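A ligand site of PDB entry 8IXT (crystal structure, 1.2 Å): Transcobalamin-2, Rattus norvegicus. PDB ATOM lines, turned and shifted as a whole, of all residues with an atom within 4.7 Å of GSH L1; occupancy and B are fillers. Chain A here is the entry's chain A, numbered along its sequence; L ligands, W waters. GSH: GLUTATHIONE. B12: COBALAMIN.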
ATOM      1  N   SER A 153      27.273  14.959  10.843  1.00  0.00           N
ATOM      2  CA  SER A 153      26.141  15.070  11.754  1.00  0.00           C
ATOM      3  C   SER A 153      25.038  15.892  11.093  1.00  0.00           C
ATOM      4  O   SER A 153      25.288  16.663  10.166  1.00  0.00           O
ATOM      5  CB  SER A 153      26.538  15.761  13.061  1.00  0.00           C
ATOM      6  OG  SER A 153      26.988  17.080  12.815  1.00  0.00           O
ATOM      7  N   TYR A 154      23.810  15.734  11.607  1.00  0.00           N
ATOM      8  CA  TYR A 154      22.750  16.656  11.221  1.00  0.00           C
ATOM      9  C   TYR A 154      23.069  18.094  11.629  1.00  0.00           C
ATOM     10  O   TYR A 154      22.571  19.025  11.000  1.00  0.00           O
ATOM     11  CB  TYR A 154      21.412  16.198  11.785  1.00  0.00           C
ATOM     12  CG  TYR A 154      20.780  15.066  10.996  1.00  0.00           C
ATOM     13  CD1 TYR A 154      20.099  15.302   9.815  1.00  0.00           C
ATOM     14  CD2 TYR A 154      20.868  13.753  11.452  1.00  0.00           C
ATOM     15  CE1 TYR A 154      19.529  14.283   9.092  1.00  0.00           C
ATOM     16  CE2 TYR A 154      20.286  12.723  10.745  1.00  0.00           C
ATOM     17  CZ  TYR A 154      19.631  12.993   9.560  1.00  0.00           C
ATOM     18  OH  TYR A 154      19.051  11.980   8.828  1.00  0.00           O
ATOM     19  N   TYR A 155      23.894  18.295  12.660  1.00  0.00           N
ATOM     20  CA  TYR A 155      24.340  19.647  13.004  1.00  0.00           C
ATOM     21  C   TYR A 155      25.097  20.265  11.839  1.00  0.00           C
ATOM     22  O   TYR A 155      24.790  21.382  11.424  1.00  0.00           O
ATOM     23  CB  TYR A 155      25.229  19.593  14.247  1.00  0.00           C
ATOM     24  CG  TYR A 155      25.720  20.948  14.726  1.00  0.00           C
ATOM     25  CD1 TYR A 155      26.865  21.518  14.187  1.00  0.00           C
ATOM     26  CD2 TYR A 155      25.051  21.644  15.723  1.00  0.00           C
ATOM     27  CE1 TYR A 155      27.336  22.729  14.626  1.00  0.00           C
ATOM     28  CE2 TYR A 155      25.512  22.872  16.172  1.00  0.00           C
ATOM     29  CZ  TYR A 155      26.656  23.417  15.617  1.00  0.00           C
ATOM     30  OH  TYR A 155      27.094  24.638  16.064  1.00  0.00           O
ATOM     31  N   PHE A 188      16.171  14.031  17.120  1.00  0.00           N
ATOM     32  CA  PHE A 188      17.124  14.590  18.064  1.00  0.00           C
ATOM     33  C   PHE A 188      16.641  14.509  19.509  1.00  0.00           C
ATOM     34  O   PHE A 188      17.267  15.085  20.409  1.00  0.00           O
ATOM     35  CB  PHE A 188      17.515  16.025  17.633  1.00  0.00           C
ATOM     36  CG  PHE A 188      17.814  16.124  16.154  1.00  0.00           C
ATOM     37  CD1 PHE A 188      18.669  15.198  15.582  1.00  0.00           C
ATOM     38  CD2 PHE A 188      17.171  17.036  15.328  1.00  0.00           C
ATOM     39  CE1 PHE A 188      18.923  15.216  14.218  1.00  0.00           C
ATOM     40  CE2 PHE A 188      17.422  17.052  13.954  1.00  0.00           C
ATOM     41  CZ  PHE A 188      18.312  16.139  13.422  1.00  0.00           C
ATOM     42  N   TYR A 190      16.228  11.735  22.504  1.00  0.00           N
ATOM     43  CA  TYR A 190      16.711  10.414  22.896  1.00  0.00           C
ATOM     44  C   TYR A 190      16.285  10.198  24.340  1.00  0.00           C
ATOM     45  O   TYR A 190      16.687  10.966  25.226  1.00  0.00           O
ATOM     46  CB  TYR A 190      18.249  10.367  22.765  1.00  0.00           C
ATOM     47  CG  TYR A 190      18.783  10.963  21.469  1.00  0.00           C
ATOM     48  CD1 TYR A 190      18.761  10.238  20.280  1.00  0.00           C
ATOM     49  CD2 TYR A 190      19.321  12.241  21.428  1.00  0.00           C
ATOM     50  CE1 TYR A 190      19.252  10.780  19.092  1.00  0.00           C
ATOM     51  CE2 TYR A 190      19.819  12.789  20.238  1.00  0.00           C
ATOM     52  CZ  TYR A 190      19.768  12.051  19.081  1.00  0.00           C
ATOM     53  OH  TYR A 190      20.244  12.581  17.900  1.00  0.00           O
ATOM     54  N   LEU A 194      15.891  16.144  24.561  1.00  0.00           N
ATOM     55  CA  LEU A 194      16.191  16.780  23.284  1.00  0.00           C
ATOM     56  C   LEU A 194      17.665  17.170  23.214  1.00  0.00           C
ATOM     57  O   LEU A 194      18.207  17.779  24.143  1.00  0.00           O
ATOM     58  CB  LEU A 194      15.340  18.032  23.111  1.00  0.00           C
ATOM     59  CG  LEU A 194      15.534  18.815  21.816  1.00  0.00           C
ATOM     60  CD1 LEU A 194      15.079  18.018  20.611  1.00  0.00           C
ATOM     61  CD2 LEU A 194      14.793  20.145  21.903  1.00  0.00           C
ATOM     62  N   SER A 195      18.299  16.841  22.092  1.00  0.00           N
ATOM     63  CA  SER A 195      19.643  17.356  21.791  1.00  0.00           C
ATOM     64  C   SER A 195      19.456  18.738  21.161  1.00  0.00           C
ATOM     65  O   SER A 195      19.271  18.880  19.945  1.00  0.00           O
ATOM     66  CB  SER A 195      20.430  16.402  20.905  1.00  0.00           C
ATOM     67  OG  SER A 195      21.810  16.650  21.092  1.00  0.00           O
ATOM     68  N   VAL A 196      19.548  19.759  21.994  1.00  0.00           N
ATOM     69  CA  VAL A 196      19.055  21.083  21.647  1.00  0.00           C
ATOM     70  C   VAL A 196      19.879  21.715  20.533  1.00  0.00           C
ATOM     71  O   VAL A 196      19.339  22.402  19.667  1.00  0.00           O
ATOM     72  CB  VAL A 196      19.005  21.952  22.914  1.00  0.00           C
ATOM     73  CG1 VAL A 196      18.792  23.390  22.567  1.00  0.00           C
ATOM     74  CG2 VAL A 196      17.936  21.437  23.865  1.00  0.00           C
ATOM     75  N   THR A 198      21.494  20.650  17.872  1.00  0.00           N
ATOM     76  CA  THR A 198      21.181  20.238  16.507  1.00  0.00           C
ATOM     77  C   THR A 198      19.779  20.695  16.123  1.00  0.00           C
ATOM     78  O   THR A 198      19.542  21.140  14.991  1.00  0.00           O
ATOM     79  CB  THR A 198      21.311  18.717  16.374  1.00  0.00           C
ATOM     80  OG1 THR A 198      22.673  18.338  16.605  1.00  0.00           O
ATOM     81  CG2 THR A 198      20.896  18.248  14.987  1.00  0.00           C
ATOM     82  N   ASN A 245      21.248  22.068  28.094  1.00  0.00           N
ATOM     83  CA  ASN A 245      22.329  22.344  29.035  1.00  0.00           C
ATOM     84  C   ASN A 245      22.818  23.748  28.761  1.00  0.00           C
ATOM     85  O   ASN A 245      22.402  24.400  27.801  1.00  0.00           O
ATOM     86  CB  ASN A 245      23.421  21.261  29.017  1.00  0.00           C
ATOM     87  CG  ASN A 245      24.259  21.237  27.753  1.00  0.00           C
ATOM     88  OD1 ASN A 245      24.642  22.255  27.204  1.00  0.00           O
ATOM     89  ND2 ASN A 245      24.613  20.032  27.332  1.00  0.00           N
HETATM   90  N1  GSH L   1      22.467  13.126  16.195  1.00  0.00           N
HETATM   91  CA1 GSH L   1      22.737  14.589  16.305  1.00  0.00           C
HETATM   92  C1  GSH L   1      23.179  15.126  14.942  1.00  0.00           C
HETATM   93  O11 GSH L   1      23.243  14.304  14.001  1.00  0.00           O
HETATM   94  O12 GSH L   1      23.473  16.346  14.869  1.00  0.00           O
HETATM   95  CB1 GSH L   1      23.840  14.866  17.323  1.00  0.00           C
HETATM   96  CG1 GSH L   1      23.500  14.462  18.757  1.00  0.00           C
HETATM   97  CD1 GSH L   1      24.740  14.522  19.618  1.00  0.00           C
HETATM   98  OE1 GSH L   1      25.792  13.994  19.270  1.00  0.00           O
HETATM   99  N2  GSH L   1      24.611  15.136  20.789  1.00  0.00           N
HETATM  100  CA2 GSH L   1      25.685  15.236  21.755  1.00  0.00           C
HETATM  101  C2  GSH L   1      25.169  15.545  23.154  1.00  0.00           C
HETATM  102  O2  GSH L   1      25.216  14.671  24.023  1.00  0.00           O
HETATM  103  CB2 GSH L   1      26.720  16.255  21.320  1.00  0.00           C
HETATM  104  SG2 GSH L   1      28.142  16.336  22.430  1.00  0.00           S
HETATM  105  N3  GSH L   1      24.585  16.728  23.339  1.00  0.00           N
HETATM  106  CA3 GSH L   1      24.141  17.166  24.649  1.00  0.00           C
HETATM  107  C3  GSH L   1      22.640  17.006  24.842  1.00  0.00           C
HETATM  108  O31 GSH L   1      22.001  16.392  23.964  1.00  0.00           O
HETATM  109  O32 GSH L   1      22.163  17.496  25.876  1.00  0.00           O
HETATM  110 CO   B12 L   2      30.067  17.218  21.268  1.00  0.00          CO
HETATM  111  N21 B12 L   2      29.945  18.778  22.325  1.00  0.00           N
HETATM  112  N22 B12 L   2      31.048  16.349  22.686  1.00  0.00           N
HETATM  113  N23 B12 L   2      30.074  15.725  20.084  1.00  0.00           N
HETATM  114  N24 B12 L   2      29.043  18.236  20.056  1.00  0.00           N
HETATM  115  C1  B12 L   2      29.441  20.003  21.682  1.00  0.00           C
HETATM  116  C20 B12 L   2      30.633  20.670  21.035  1.00  0.00           C
HETATM  117  C2  B12 L   2      28.788  20.780  22.892  1.00  0.00           C
HETATM  118  C25 B12 L   2      28.709  22.308  22.699  1.00  0.00           C
HETATM  119  C26 B12 L   2      27.354  20.258  23.136  1.00  0.00           C
HETATM  120  C27 B12 L   2      26.680  20.689  24.420  1.00  0.00           C
HETATM  121  O28 B12 L   2      26.915  20.105  25.473  1.00  0.00           O
HETATM  122  N29 B12 L   2      25.856  21.713  24.337  1.00  0.00           N
HETATM  123  C3  B12 L   2      29.719  20.335  24.082  1.00  0.00           C
HETATM  124  C30 B12 L   2      30.945  21.218  24.350  1.00  0.00           C
HETATM  125  C31 B12 L   2      30.675  22.306  25.395  1.00  0.00           C
HETATM  126  C32 B12 L   2      31.917  23.065  25.799  1.00  0.00           C
HETATM  127  O34 B12 L   2      32.919  23.111  25.076  1.00  0.00           O
HETATM  128  N33 B12 L   2      31.860  23.661  26.973  1.00  0.00           N
HETATM  129  C4  B12 L   2      30.124  18.967  23.593  1.00  0.00           C
HETATM  130  C5  B12 L   2      30.710  17.954  24.468  1.00  0.00           C
HETATM  131  C35 B12 L   2      30.793  18.353  25.915  1.00  0.00           C
HETATM  132  C6  B12 L   2      31.208  16.766  24.001  1.00  0.00           C
HETATM  133  C7  B12 L   2      31.929  15.686  24.805  1.00  0.00           C
HETATM  134  C36 B12 L   2      33.038  16.245  25.724  1.00  0.00           C
HETATM  135  C37 B12 L   2      30.861  14.958  25.639  1.00  0.00           C
HETATM  136  C38 B12 L   2      31.468  13.906  26.578  1.00  0.00           C
HETATM  137  O39 B12 L   2      32.171  12.975  26.180  1.00  0.00           O
HETATM  138  N40 B12 L   2      31.175  14.095  27.849  1.00  0.00           N
HETATM  139  C8  B12 L   2      32.466  14.731  23.707  1.00  0.00           C
HETATM  140  C41 B12 L   2      33.936  14.876  23.272  1.00  0.00           C
HETATM  141  C42 B12 L   2      34.920  14.101  24.151  1.00  0.00           C
HETATM  142  C43 B12 L   2      36.208  13.840  23.393  1.00  0.00           C
HETATM  143  O44 B12 L   2      37.054  14.739  23.261  1.00  0.00           O
HETATM  144  N45 B12 L   2      36.358  12.626  22.876  1.00  0.00           N
HETATM  145  C9  B12 L   2      31.593  15.106  22.545  1.00  0.00           C
HETATM  146  C10 B12 L   2      31.310  14.235  21.516  1.00  0.00           C
HETATM  147  C11 B12 L   2      30.549  14.492  20.408  1.00  0.00           C
HETATM  148  C12 B12 L   2      30.150  13.474  19.368  1.00  0.00           C
HETATM  149  C46 B12 L   2      31.195  12.376  19.134  1.00  0.00           C
HETATM  150  C47 B12 L   2      28.849  12.828  19.883  1.00  0.00           C
HETATM  151  C13 B12 L   2      29.887  14.358  18.115  1.00  0.00           C
HETATM  152  C48 B12 L   2      31.095  14.557  17.184  1.00  0.00           C
HETATM  153  C49 B12 L   2      31.293  13.462  16.151  1.00  0.00           C
HETATM  154  C50 B12 L   2      30.536  13.717  14.872  1.00  0.00           C
HETATM  155  O51 B12 L   2      30.658  14.783  14.265  1.00  0.00           O
HETATM  156  N52 B12 L   2      29.769  12.742  14.433  1.00  0.00           N
HETATM  157  C14 B12 L   2      29.588  15.713  18.776  1.00  0.00           C
HETATM  158  C15 B12 L   2      28.940  16.740  18.151  1.00  0.00           C
HETATM  159  C53 B12 L   2      28.403  16.547  16.767  1.00  0.00           C
HETATM  160  C16 B12 L   2      28.694  18.035  18.819  1.00  0.00           C
HETATM  161  C17 B12 L   2      27.933  19.214  18.230  1.00  0.00           C
HETATM  162  C54 B12 L   2      26.440  18.837  18.251  1.00  0.00           C
HETATM  163  C55 B12 L   2      28.305  19.683  16.805  1.00  0.00           C
HETATM  164  C56 B12 L   2      29.813  19.810  16.596  1.00  0.00           C
HETATM  165  C57 B12 L   2      30.105  20.212  15.177  1.00  0.00           C
HETATM  166  O58 B12 L   2      29.944  19.425  14.233  1.00  0.00           O
HETATM  167  N59 B12 L   2      30.495  21.466  14.984  1.00  0.00           N
HETATM  168  C18 B12 L   2      28.294  20.318  19.254  1.00  0.00           C
HETATM  169  C60 B12 L   2      27.230  21.436  19.309  1.00  0.00           C
HETATM  170  C61 B12 L   2      27.730  22.869  19.408  1.00  0.00           C
HETATM  171  O63 B12 L   2      28.823  23.186  18.924  1.00  0.00           O
HETATM  172  N62 B12 L   2      26.920  23.742  19.977  1.00  0.00           N
HETATM  173  C19 B12 L   2      28.490  19.520  20.553  1.00  0.00           C
HETATM  174  C1P B12 L   2      30.807  22.022  13.677  1.00  0.00           C
HETATM  175  C2P B12 L   2      32.199  21.563  13.139  1.00  0.00           C
HETATM  176  C3P B12 L   2      32.457  22.168  11.775  1.00  0.00           C
HETATM  177  O3  B12 L   2      33.169  21.979  14.096  1.00  0.00           O
HETATM  178  O4  B12 L   2      35.206  20.756  13.283  1.00  0.00           O
HETATM  179  O5  B12 L   2      35.110  21.610  15.650  1.00  0.00           O
HETATM  180  P   B12 L   2      34.369  21.045  14.463  1.00  0.00           P
HETATM  181  O2  B12 L   2      33.551  19.750  14.888  1.00  0.00           O
HETATM  182  C3R B12 L   2      34.162  18.737  15.669  1.00  0.00           C
HETATM  183  C2R B12 L   2      34.215  19.031  17.157  1.00  0.00           C
HETATM  184  O7R B12 L   2      32.955  19.540  17.592  1.00  0.00           O
HETATM  185  C1R B12 L   2      34.362  17.620  17.709  1.00  0.00           C
HETATM  186  O6R B12 L   2      33.703  16.756  16.812  1.00  0.00           O
HETATM  187  C4R B12 L   2      33.333  17.470  15.614  1.00  0.00           C
HETATM  188  C5R B12 L   2      33.577  16.603  14.406  1.00  0.00           C
HETATM  189  O8R B12 L   2      34.952  16.252  14.298  1.00  0.00           O
HETATM  190  N1B B12 L   2      33.745  17.487  19.013  1.00  0.00           N
HETATM  191  C8B B12 L   2      34.276  18.037  20.170  1.00  0.00           C
HETATM  192  C2B B12 L   2      32.410  17.346  19.238  1.00  0.00           C
HETATM  193  N3B B12 L   2      32.039  17.707  20.445  1.00  0.00           N
HETATM  194  C9B B12 L   2      33.202  18.171  21.037  1.00  0.00           C
HETATM  195  C4B B12 L   2      33.410  18.747  22.295  1.00  0.00           C
HETATM  196  C5B B12 L   2      34.677  19.192  22.658  1.00  0.00           C
HETATM  197  C5M B12 L   2      34.847  19.904  23.965  1.00  0.00           C
HETATM  198  C6B B12 L   2      35.755  19.037  21.762  1.00  0.00           C
HETATM  199  C6M B12 L   2      37.140  19.488  22.120  1.00  0.00           C
HETATM  200  C7B B12 L   2      35.543  18.456  20.516  1.00  0.00           C
HETATM  201  O   HOH W   1      23.360  17.667  28.490  1.00  0.00           O
HETATM  202  O   HOH W   2      26.600  12.182  17.431  1.00  0.00           O
HETATM  203  O   HOH W   3      28.203  13.302  23.636  1.00  0.00           O
HETATM  204  O   HOH W   4      27.377  17.383  25.479  1.00  0.00           O
HETATM  205  O   HOH W   5      21.010  19.792  24.748  1.00  0.00           O
HETATM  206  O   HOH W   6      24.582  18.807  21.413  1.00  0.00           O
HETATM  207  O   HOH W   7      20.279  11.802  14.550  1.00  0.00           O
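CB of Ser 153 touches O12 of GSH L1, at 3.6 Å. ND2 of Asn 245 touches O32 of GSH L1, 3.8 Å away. Seven residues have an atom within 4 Å of GSH L1: Ser 153, Tyr 154, Tyr 155, Tyr 190, Ser 195, Thr 198 and Asn 245. The nearest printed residue that does not touch GSH L1 is Leu 194 (4.04 Å).
A cobalt atom (CO) of B12 L2 is bound by a sulfur (SG2) of GSH L1 (2.4 Å).
Water W5 bridges an oxygen (O32) of GSH L1 (2.8 Å) and the backbone NH of Val 196 (3.1 Å). Water W1 lies within hydrogen-bond range of O32 of GSH L1 (2.9 Å) and ND2 of Asn 245 (2.9 Å). Water W7 lies within hydrogen-bond range of a nitrogen (N1) of GSH L1 (3.0 Å) and the side-chain hydroxyl (OH) of Tyr 190 (3.4 Å).
N of Tyr 154 is in hydrogen-bond range of O11 of GSH L1 (2.8 Å). The side-chain hydroxyl of Thr 198 is in hydrogen-bond range of an oxygen (O12) of GSH L1 (2.8 Å). O28 of B12 L2 is in hydrogen-bond range of ND2 of Asn 245 (3.0 Å). O31 of GSH L1 lies within hydrogen-bond range of OG of Ser 195 (2.9 Å). A nitrogen (N1) of GSH L1 lies within hydrogen-bond range of the side-chain hydroxyl (OH) of Tyr 190 (2.9 Å). The backbone NH (N) of Tyr 155 lies within hydrogen-bond range of an oxygen (O12) of GSH L1 (3.0 Å).
The backbone NH (N) of Tyr 155 lies close to the side-chain hydroxyl (OG) of Ser 153, at 3.3 Å. The backbone NH of Ser 195 is in hydrogen-bond range of the backbone carbonyl oxygen of Phe 188 (2.6 Å).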
